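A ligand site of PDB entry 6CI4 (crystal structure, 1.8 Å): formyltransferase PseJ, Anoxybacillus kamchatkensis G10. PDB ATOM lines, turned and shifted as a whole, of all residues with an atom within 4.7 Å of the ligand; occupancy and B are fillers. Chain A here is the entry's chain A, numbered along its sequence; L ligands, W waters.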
ATOM      1  N   GLY A  73       9.970  31.228 -10.671  1.00  0.00           N
ATOM      2  CA  GLY A  73       9.952  30.488  -9.417  1.00  0.00           C
ATOM      3  C   GLY A  73       8.563  30.056  -9.013  1.00  0.00           C
ATOM      4  O   GLY A  73       8.383  29.570  -7.896  1.00  0.00           O
ATOM      5  N   TYR A  74       7.586  30.245  -9.880  1.00  0.00           N
ATOM      6  CA  TYR A  74       6.217  29.872  -9.574  1.00  0.00           C
ATOM      7  C   TYR A  74       6.126  28.355  -9.586  1.00  0.00           C
ATOM      8  O   TYR A  74       6.752  27.684 -10.410  1.00  0.00           O
ATOM      9  CB  TYR A  74       5.295  30.528 -10.587  1.00  0.00           C
ATOM     10  CG  TYR A  74       3.802  30.441 -10.257  1.00  0.00           C
ATOM     11  CD1 TYR A  74       2.918  29.904 -11.173  1.00  0.00           C
ATOM     12  CD2 TYR A  74       3.283  30.894  -9.052  1.00  0.00           C
ATOM     13  CE1 TYR A  74       1.569  29.824 -10.924  1.00  0.00           C
ATOM     14  CE2 TYR A  74       1.902  30.810  -8.765  1.00  0.00           C
ATOM     15  CZ  TYR A  74       1.064  30.277  -9.710  1.00  0.00           C
ATOM     16  OH  TYR A  74      -0.289  30.176  -9.473  1.00  0.00           O
ATOM     17  N   ARG A  75       5.389  27.805  -8.627  1.00  0.00           N
ATOM     18  CA  ARG A  75       5.400  26.367  -8.384  1.00  0.00           C
ATOM     19  C   ARG A  75       4.103  25.690  -8.783  1.00  0.00           C
ATOM     20  O   ARG A  75       3.894  24.521  -8.443  1.00  0.00           O
ATOM     21  CB  ARG A  75       5.727  26.097  -6.921  1.00  0.00           C
ATOM     22  CG  ARG A  75       7.072  26.722  -6.455  1.00  0.00           C
ATOM     23  CD  ARG A  75       7.611  26.073  -5.179  1.00  0.00           C
ATOM     24  NE  ARG A  75       7.945  24.668  -5.392  1.00  0.00           N
ATOM     25  CZ  ARG A  75       9.102  24.217  -5.866  1.00  0.00           C
ATOM     26  NH1 ARG A  75      10.086  25.048  -6.212  1.00  0.00           N
ATOM     27  NH2 ARG A  75       9.282  22.911  -6.004  1.00  0.00           N
ATOM     28  N   ASN A  92       8.298  33.609 -18.850  1.00  0.00           N
ATOM     29  CA  ASN A  92       8.806  32.776 -17.772  1.00  0.00           C
ATOM     30  C   ASN A  92      10.322  32.866 -17.815  1.00  0.00           C
ATOM     31  O   ASN A  92      10.893  32.947 -18.897  1.00  0.00           O
ATOM     32  CB  ASN A  92       8.307  31.329 -17.920  1.00  0.00           C
ATOM     33  CG  ASN A  92       8.788  30.426 -16.816  1.00  0.00           C
ATOM     34  OD1 ASN A  92       8.610  30.724 -15.629  1.00  0.00           O
ATOM     35  ND2 ASN A  92       9.402  29.308 -17.194  1.00  0.00           N
ATOM     36  N   HIS A  94      13.341  30.758 -16.808  1.00  0.00           N
ATOM     37  CA  HIS A  94      13.586  29.354 -16.544  1.00  0.00           C
ATOM     38  C   HIS A  94      15.070  29.081 -16.639  1.00  0.00           C
ATOM     39  O   HIS A  94      15.680  29.354 -17.663  1.00  0.00           O
ATOM     40  CB  HIS A  94      12.815  28.527 -17.561  1.00  0.00           C
ATOM     41  CG  HIS A  94      12.953  27.060 -17.369  1.00  0.00           C
ATOM     42  ND1 HIS A  94      12.364  26.396 -16.310  1.00  0.00           N
ATOM     43  CD2 HIS A  94      13.613  26.115 -18.083  1.00  0.00           C
ATOM     44  CE1 HIS A  94      12.650  25.113 -16.378  1.00  0.00           C
ATOM     45  NE2 HIS A  94      13.411  24.916 -17.449  1.00  0.00           N
ATOM     46  N   ILE A  95      15.642  28.491 -15.597  1.00  0.00           N
ATOM     47  CA  ILE A  95      17.085  28.345 -15.517  1.00  0.00           C
ATOM     48  C   ILE A  95      17.526  27.047 -16.161  1.00  0.00           C
ATOM     49  O   ILE A  95      18.335  26.293 -15.605  1.00  0.00           O
ATOM     50  CB  ILE A  95      17.595  28.470 -14.064  1.00  0.00           C
ATOM     51  CG1 ILE A  95      16.889  27.528 -13.114  1.00  0.00           C
ATOM     52  CG2 ILE A  95      17.469  29.904 -13.602  1.00  0.00           C
ATOM     53  CD1 ILE A  95      17.728  27.256 -11.804  1.00  0.00           C
ATOM     54  N   GLY A 103      10.652  21.777 -17.091  1.00  0.00           N
ATOM     55  CA  GLY A 103      10.108  21.203 -15.867  1.00  0.00           C
ATOM     56  C   GLY A 103      10.970  21.375 -14.622  1.00  0.00           C
ATOM     57  O   GLY A 103      11.569  22.432 -14.411  1.00  0.00           O
ATOM     58  N   ALA A 104      11.110  20.313 -13.837  1.00  0.00           N
ATOM     59  CA  ALA A 104      11.625  20.406 -12.491  1.00  0.00           C
ATOM     60  C   ALA A 104      13.136  20.132 -12.398  1.00  0.00           C
ATOM     61  O   ALA A 104      13.702  19.373 -13.186  1.00  0.00           O
ATOM     62  CB  ALA A 104      10.856  19.410 -11.600  1.00  0.00           C
ATOM     63  N   ASP A 105      13.766  20.749 -11.389  1.00  0.00           N
ATOM     64  CA  ASP A 105      15.148  20.509 -11.000  1.00  0.00           C
ATOM     65  C   ASP A 105      16.075  20.592 -12.201  1.00  0.00           C
ATOM     66  O   ASP A 105      16.926  19.714 -12.415  1.00  0.00           O
ATOM     67  CB  ASP A 105      15.243  19.139 -10.327  1.00  0.00           C
ATOM     68  CG  ASP A 105      14.307  19.023  -9.131  1.00  0.00           C
ATOM     69  OD1 ASP A 105      14.393  19.846  -8.181  1.00  0.00           O
ATOM     70  OD2 ASP A 105      13.469  18.123  -9.155  1.00  0.00           O
ATOM     71  N   PRO A 106      15.933  21.606 -13.063  1.00  0.00           N
ATOM     72  CA  PRO A 106      16.769  21.587 -14.273  1.00  0.00           C
ATOM     73  C   PRO A 106      18.250  21.539 -13.999  1.00  0.00           C
ATOM     74  O   PRO A 106      18.990  20.866 -14.764  1.00  0.00           O
ATOM     75  CB  PRO A 106      16.377  22.874 -15.015  1.00  0.00           C
ATOM     76  CG  PRO A 106      15.794  23.756 -13.952  1.00  0.00           C
ATOM     77  CD  PRO A 106      15.031  22.757 -13.048  1.00  0.00           C
ATOM     78  N   ASN A 107      18.745  22.257 -12.995  1.00  0.00           N
ATOM     79  CA  ASN A 107      20.197  22.260 -12.766  1.00  0.00           C
ATOM     80  C   ASN A 107      20.682  20.849 -12.496  1.00  0.00           C
ATOM     81  O   ASN A 107      21.640  20.365 -13.127  1.00  0.00           O
ATOM     82  CB  ASN A 107      20.548  23.186 -11.597  1.00  0.00           C
ATOM     83  CG  ASN A 107      22.036  23.349 -11.405  1.00  0.00           C
ATOM     84  OD1 ASN A 107      22.766  23.563 -12.365  1.00  0.00           O
ATOM     85  ND2 ASN A 107      22.498  23.248 -10.161  1.00  0.00           N
ATOM     86  N   LEU A 108      20.003  20.148 -11.590  1.00  0.00           N
ATOM     87  CA  LEU A 108      20.394  18.781 -11.256  1.00  0.00           C
ATOM     88  C   LEU A 108      20.411  17.907 -12.502  1.00  0.00           C
ATOM     89  O   LEU A 108      21.419  17.248 -12.826  1.00  0.00           O
ATOM     90  CB  LEU A 108      19.429  18.214 -10.202  1.00  0.00           C
ATOM     91  CG  LEU A 108      19.662  16.747  -9.862  1.00  0.00           C
ATOM     92  CD1 LEU A 108      21.079  16.463  -9.398  1.00  0.00           C
ATOM     93  CD2 LEU A 108      18.608  16.290  -8.801  1.00  0.00           C
ATOM     94  N   LEU A 147      26.217  21.684  -6.693  1.00  0.00           N
ATOM     95  CA  LEU A 147      24.865  22.030  -7.115  1.00  0.00           C
ATOM     96  C   LEU A 147      24.461  23.413  -6.650  1.00  0.00           C
ATOM     97  O   LEU A 147      23.621  24.056  -7.294  1.00  0.00           O
ATOM     98  CB  LEU A 147      23.850  21.004  -6.591  1.00  0.00           C
ATOM     99  CG  LEU A 147      23.837  19.680  -7.343  1.00  0.00           C
ATOM    100  CD1 LEU A 147      22.929  18.677  -6.638  1.00  0.00           C
ATOM    101  CD2 LEU A 147      23.417  19.840  -8.833  1.00  0.00           C
ATOM    102  N   ARG A 148      25.045  23.872  -5.525  1.00  0.00           N
ATOM    103  CA  ARG A 148      24.721  25.203  -5.007  1.00  0.00           C
ATOM    104  C   ARG A 148      25.407  26.287  -5.836  1.00  0.00           C
ATOM    105  O   ARG A 148      24.780  27.305  -6.179  1.00  0.00           O
ATOM    106  CB  ARG A 148      25.137  25.281  -3.523  1.00  0.00           C
ATOM    107  CG  ARG A 148      25.183  26.655  -2.877  1.00  0.00           C
ATOM    108  CD  ARG A 148      24.204  26.836  -1.781  1.00  0.00           C
ATOM    109  NE  ARG A 148      24.207  25.770  -0.748  1.00  0.00           N
ATOM    110  CZ  ARG A 148      23.087  25.330  -0.182  1.00  0.00           C
ATOM    111  NH1 ARG A 148      21.913  25.868  -0.546  1.00  0.00           N
ATOM    112  NH2 ARG A 148      23.120  24.358   0.734  1.00  0.00           N
ATOM    113  N   TYR A 151      23.775  26.479  -9.316  1.00  0.00           N
ATOM    114  CA  TYR A 151      22.431  27.064  -9.241  1.00  0.00           C
ATOM    115  C   TYR A 151      22.511  28.571  -9.033  1.00  0.00           C
ATOM    116  O   TYR A 151      21.741  29.324  -9.648  1.00  0.00           O
ATOM    117  CB  TYR A 151      21.635  26.408  -8.090  1.00  0.00           C
ATOM    118  CG  TYR A 151      20.231  27.001  -7.937  1.00  0.00           C
ATOM    119  CD1 TYR A 151      19.138  26.352  -8.456  1.00  0.00           C
ATOM    120  CD2 TYR A 151      20.034  28.203  -7.264  1.00  0.00           C
ATOM    121  CE1 TYR A 151      17.847  26.871  -8.319  1.00  0.00           C
ATOM    122  CE2 TYR A 151      18.781  28.729  -7.112  1.00  0.00           C
ATOM    123  CZ  TYR A 151      17.682  28.054  -7.651  1.00  0.00           C
ATOM    124  OH  TYR A 151      16.405  28.574  -7.505  1.00  0.00           O
ATOM    125  N   GLU A 152      23.415  29.038  -8.162  1.00  0.00           N
ATOM    126  CA  GLU A 152      23.533  30.474  -7.911  1.00  0.00           C
ATOM    127  C   GLU A 152      24.072  31.199  -9.131  1.00  0.00           C
ATOM    128  O   GLU A 152      23.686  32.339  -9.409  1.00  0.00           O
ATOM    129  CB  GLU A 152      24.450  30.736  -6.715  1.00  0.00           C
ATOM    130  CG  GLU A 152      23.924  30.166  -5.394  1.00  0.00           C
ATOM    131  CD  GLU A 152      22.573  30.763  -4.967  1.00  0.00           C
ATOM    132  OE1 GLU A 152      21.935  30.191  -4.060  1.00  0.00           O
ATOM    133  OE2 GLU A 152      22.143  31.788  -5.553  1.00  0.00           O
ATOM    134  N   LEU A 188       9.062  16.478 -10.728  1.00  0.00           N
ATOM    135  CA  LEU A 188       9.696  16.521  -9.412  1.00  0.00           C
ATOM    136  C   LEU A 188      10.121  15.145  -8.919  1.00  0.00           C
ATOM    137  O   LEU A 188      11.177  14.992  -8.289  1.00  0.00           O
ATOM    138  CB  LEU A 188       8.743  17.150  -8.405  1.00  0.00           C
ATOM    139  CG  LEU A 188       8.778  18.659  -8.329  1.00  0.00           C
ATOM    140  CD1 LEU A 188       7.637  19.109  -7.420  1.00  0.00           C
ATOM    141  CD2 LEU A 188      10.128  19.086  -7.798  1.00  0.00           C
ATOM    142  N   TRP A 202      22.686  20.274  -1.546  1.00  0.00           N
ATOM    143  CA  TRP A 202      23.072  21.131  -2.674  1.00  0.00           C
ATOM    144  C   TRP A 202      24.564  21.403  -2.727  1.00  0.00           C
ATOM    145  O   TRP A 202      25.043  21.875  -3.772  1.00  0.00           O
ATOM    146  CB  TRP A 202      22.284  22.447  -2.627  1.00  0.00           C
ATOM    147  CG  TRP A 202      20.781  22.286  -2.650  1.00  0.00           C
ATOM    148  CD1 TRP A 202      19.865  22.839  -1.755  1.00  0.00           C
ATOM    149  CD2 TRP A 202      20.015  21.501  -3.553  1.00  0.00           C
ATOM    150  NE1 TRP A 202      18.587  22.442  -2.093  1.00  0.00           N
ATOM    151  CE2 TRP A 202      18.651  21.636  -3.198  1.00  0.00           C
ATOM    152  CE3 TRP A 202      20.342  20.693  -4.645  1.00  0.00           C
ATOM    153  CZ2 TRP A 202      17.631  20.983  -3.889  1.00  0.00           C
ATOM    154  CZ3 TRP A 202      19.306  20.059  -5.355  1.00  0.00           C
ATOM    155  CH2 TRP A 202      17.973  20.210  -4.954  1.00  0.00           C
HETATM  156  C1  LIG L   1      15.129  25.771  -3.806  1.00  0.00           C
HETATM  157  C2  LIG L   1      17.275  27.194  -4.292  1.00  0.00           C
HETATM  158  C3  LIG L   1      18.690  25.590  -3.586  1.00  0.00           C
HETATM  159  C4  LIG L   1      20.044  23.297  -6.944  1.00  0.00           C
HETATM  160  C5  LIG L   1      18.619  23.255  -6.585  1.00  0.00           C
HETATM  161  C6  LIG L   1      10.582  26.057 -12.114  1.00  0.00           C
HETATM  162  C7  LIG L   1      11.980  26.567 -11.841  1.00  0.00           C
HETATM  163  C8  LIG L   1      12.982  26.199 -12.903  1.00  0.00           C
HETATM  164  C9  LIG L   1      11.640  26.482  -9.500  1.00  0.00           C
HETATM  165  C10 LIG L   1      16.486  26.175  -3.253  1.00  0.00           C
HETATM  166  C11 LIG L   1      18.522  27.137  -3.927  1.00  0.00           C
HETATM  167  C12 LIG L   1      20.555  24.904  -4.996  1.00  0.00           C
HETATM  168  C13 LIG L   1      18.151  24.058  -5.469  1.00  0.00           C
HETATM  169  C14 LIG L   1      10.196  26.011  -9.676  1.00  0.00           C
HETATM  170  C15 LIG L   1       9.050  23.715  -9.440  1.00  0.00           C
HETATM  171  C16 LIG L   1       9.193  22.198  -9.482  1.00  0.00           C
HETATM  172  C17 LIG L   1       9.667  26.377 -11.002  1.00  0.00           C
HETATM  173  N1  LIG L   1      10.230  26.785 -13.343  1.00  0.00           N
HETATM  174  N2  LIG L   1      19.087  24.854  -4.675  1.00  0.00           N
HETATM  175  N3  LIG L   1      20.962  24.052  -6.161  1.00  0.00           N
HETATM  176  N4  LIG L   1      10.240  24.513  -9.674  1.00  0.00           N
HETATM  177  O1  LIG L   1      12.470  25.985 -10.573  1.00  0.00           O
HETATM  178  O2  LIG L   1      12.138  25.995  -8.346  1.00  0.00           O
HETATM  179  O3  LIG L   1      14.431  27.197  -8.656  1.00  0.00           O
HETATM  180  O4  LIG L   1      13.789  26.311  -6.329  1.00  0.00           O
HETATM  181  O5  LIG L   1      15.360  25.073  -5.056  1.00  0.00           O
HETATM  182  O6  LIG L   1      20.480  22.688  -7.863  1.00  0.00           O
HETATM  183  O7  LIG L   1      21.297  25.538  -4.396  1.00  0.00           O
HETATM  184  O8  LIG L   1      17.298  25.156  -3.125  1.00  0.00           O
HETATM  185  O9  LIG L   1      18.807  28.003  -2.768  1.00  0.00           O
HETATM  186  O10 LIG L   1      16.721  28.521  -4.191  1.00  0.00           O
HETATM  187  O11 LIG L   1      14.774  24.124  -7.392  1.00  0.00           O
HETATM  188  O12 LIG L   1      13.051  24.017  -5.455  1.00  0.00           O
HETATM  189  O13 LIG L   1      12.570  28.294  -7.418  1.00  0.00           O
HETATM  190  O14 LIG L   1       8.026  24.264  -9.228  1.00  0.00           O
HETATM  191  O15 LIG L   1       9.397  27.812 -11.044  1.00  0.00           O
HETATM  192  P1  LIG L   1      13.250  26.994  -7.699  1.00  0.00           P
HETATM  193  P2  LIG L   1      14.179  24.748  -6.121  1.00  0.00           P
HETATM  194  O   HOH W   1      14.918  24.621  -9.979  1.00  0.00           O
HETATM  195  O   HOH W   2      12.629  22.943  -9.858  1.00  0.00           O
HETATM  196  O   HOH W   3      19.200  30.502  -3.593  1.00  0.00           O
HETATM  197  O   HOH W   4      13.125  30.667  -8.764  1.00  0.00           O
HETATM  198  O   HOH W   5       9.581  24.431 -14.764  1.00  0.00           O
HETATM  199  O   HOH W   6      14.748  29.379 -10.515  1.00  0.00           O
HETATM  200  O   HOH W   7      10.665  29.852 -13.211  1.00  0.00           O
HETATM  201  O   HOH W   8      14.370  29.709  -5.466  1.00  0.00           O
HETATM  202  O   HOH W   9      11.953  22.165  -7.011  1.00  0.00           O
HETATM  203  O   HOH W  10       6.005  22.767  -8.547  1.00  0.00           O
HETATM  204  O   HOH W  11      10.124  28.242  -6.244  1.00  0.00           O
HETATM  205  O   HOH W  12      21.459  28.258  -2.267  1.00  0.00           O
HETATM  206  O   HOH W  13       7.767  29.755 -12.908  1.00  0.00           O
HETATM  207  O   HOH W  14      13.924  29.350 -13.267  1.00  0.00           O
HETATM  208  O   HOH W  15      18.478  21.592  -9.375  1.00  0.00           O
HETATM  209  O   HOH W  16      16.044  21.755  -7.907  1.00  0.00           O
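His 94 touches the ligand. Ala 104 touches the ligand (CB to C16, 3.9 Å). CG of Pro 106 touches C8 of the ligand (3.9 Å). Arg 148 touches the ligand (CA to O7, 3.5 Å). Leu 188 touches the ligand (CD2 to C16, 3.7 Å). Hydrophobic or aromatic side chains within 4 Å of the ligand: His 94, Ala 104, Pro 106, Leu 147, Tyr 151, Leu 188 and Trp 202.
OH of Tyr 151 lies within hydrogen-bond range of O3 of the ligand, at 2.7 Å. N of Tyr 74 lies within hydrogen-bond range of O15 of the ligand (3.2 Å). An oxygen (O15) of the ligand sits at hydrogen-bond distance from the backbone carbonyl oxygen of Tyr 74 (2.7 Å). O of Leu 147 lies within hydrogen-bond range of N3 of the ligand, 2.9 Å away. The guanidinium group (NH1) of Arg 75 is in salt-bridge range of an oxygen (O12) of the ligand, 3.2 Å away. ND2 of Asn 107 sits at hydrogen-bond distance from O6 of the ligand (3.1 Å). An oxygen (O15) of the ligand sits close to the backbone NH (N) of Gly 73 (3.5 Å). NE1 of Trp 202 lies within hydrogen-bond range of O8 of the ligand (3.2 Å).
Water W9 lies within hydrogen-bond range of O12 of the ligand (2.7 Å) and NH2 of Arg 75 (3.0 Å). Water W11 lies within hydrogen-bond range of an oxygen (O13) of the ligand (2.7 Å), the backbone carbonyl oxygen of Gly 73 (2.7 Å) and the guanidinium group of Arg 75 (3.2 Å). Water W16 bridges the side-chain carboxylate of Asp 105 and an oxygen (O11) of the ligand. Water W5 bridges N1 of the ligand and O of Gly 103. Water W8 lies within hydrogen-bond range of an oxygen (O10) of the ligand (2.9 Å) and the side-chain hydroxyl (OH) of Tyr 151 (3.1 Å). Water W13 lies within hydrogen-bond range of the side-chain amide oxygen (OD1) of Asn 92 (3.0 Å), the backbone NH (N) of Tyr 74 (3.1 Å), an oxygen (O15) of the ligand (3.1 Å) and the backbone NH (N) of Gly 73 (3.5 Å).
The backbone carbonyl oxygen (O) of Leu 147 sits at hydrogen-bond distance from the side-chain amide nitrogen (ND2) of Asn 107 (3.2 Å). The backbone NH (N) of Leu 147 is in hydrogen-bond range of the backbone carbonyl oxygen (O) of Trp 202, at 3.2 Å. N of Arg 148 sits at hydrogen-bond distance from O of Trp 202, at 2.7 Å.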
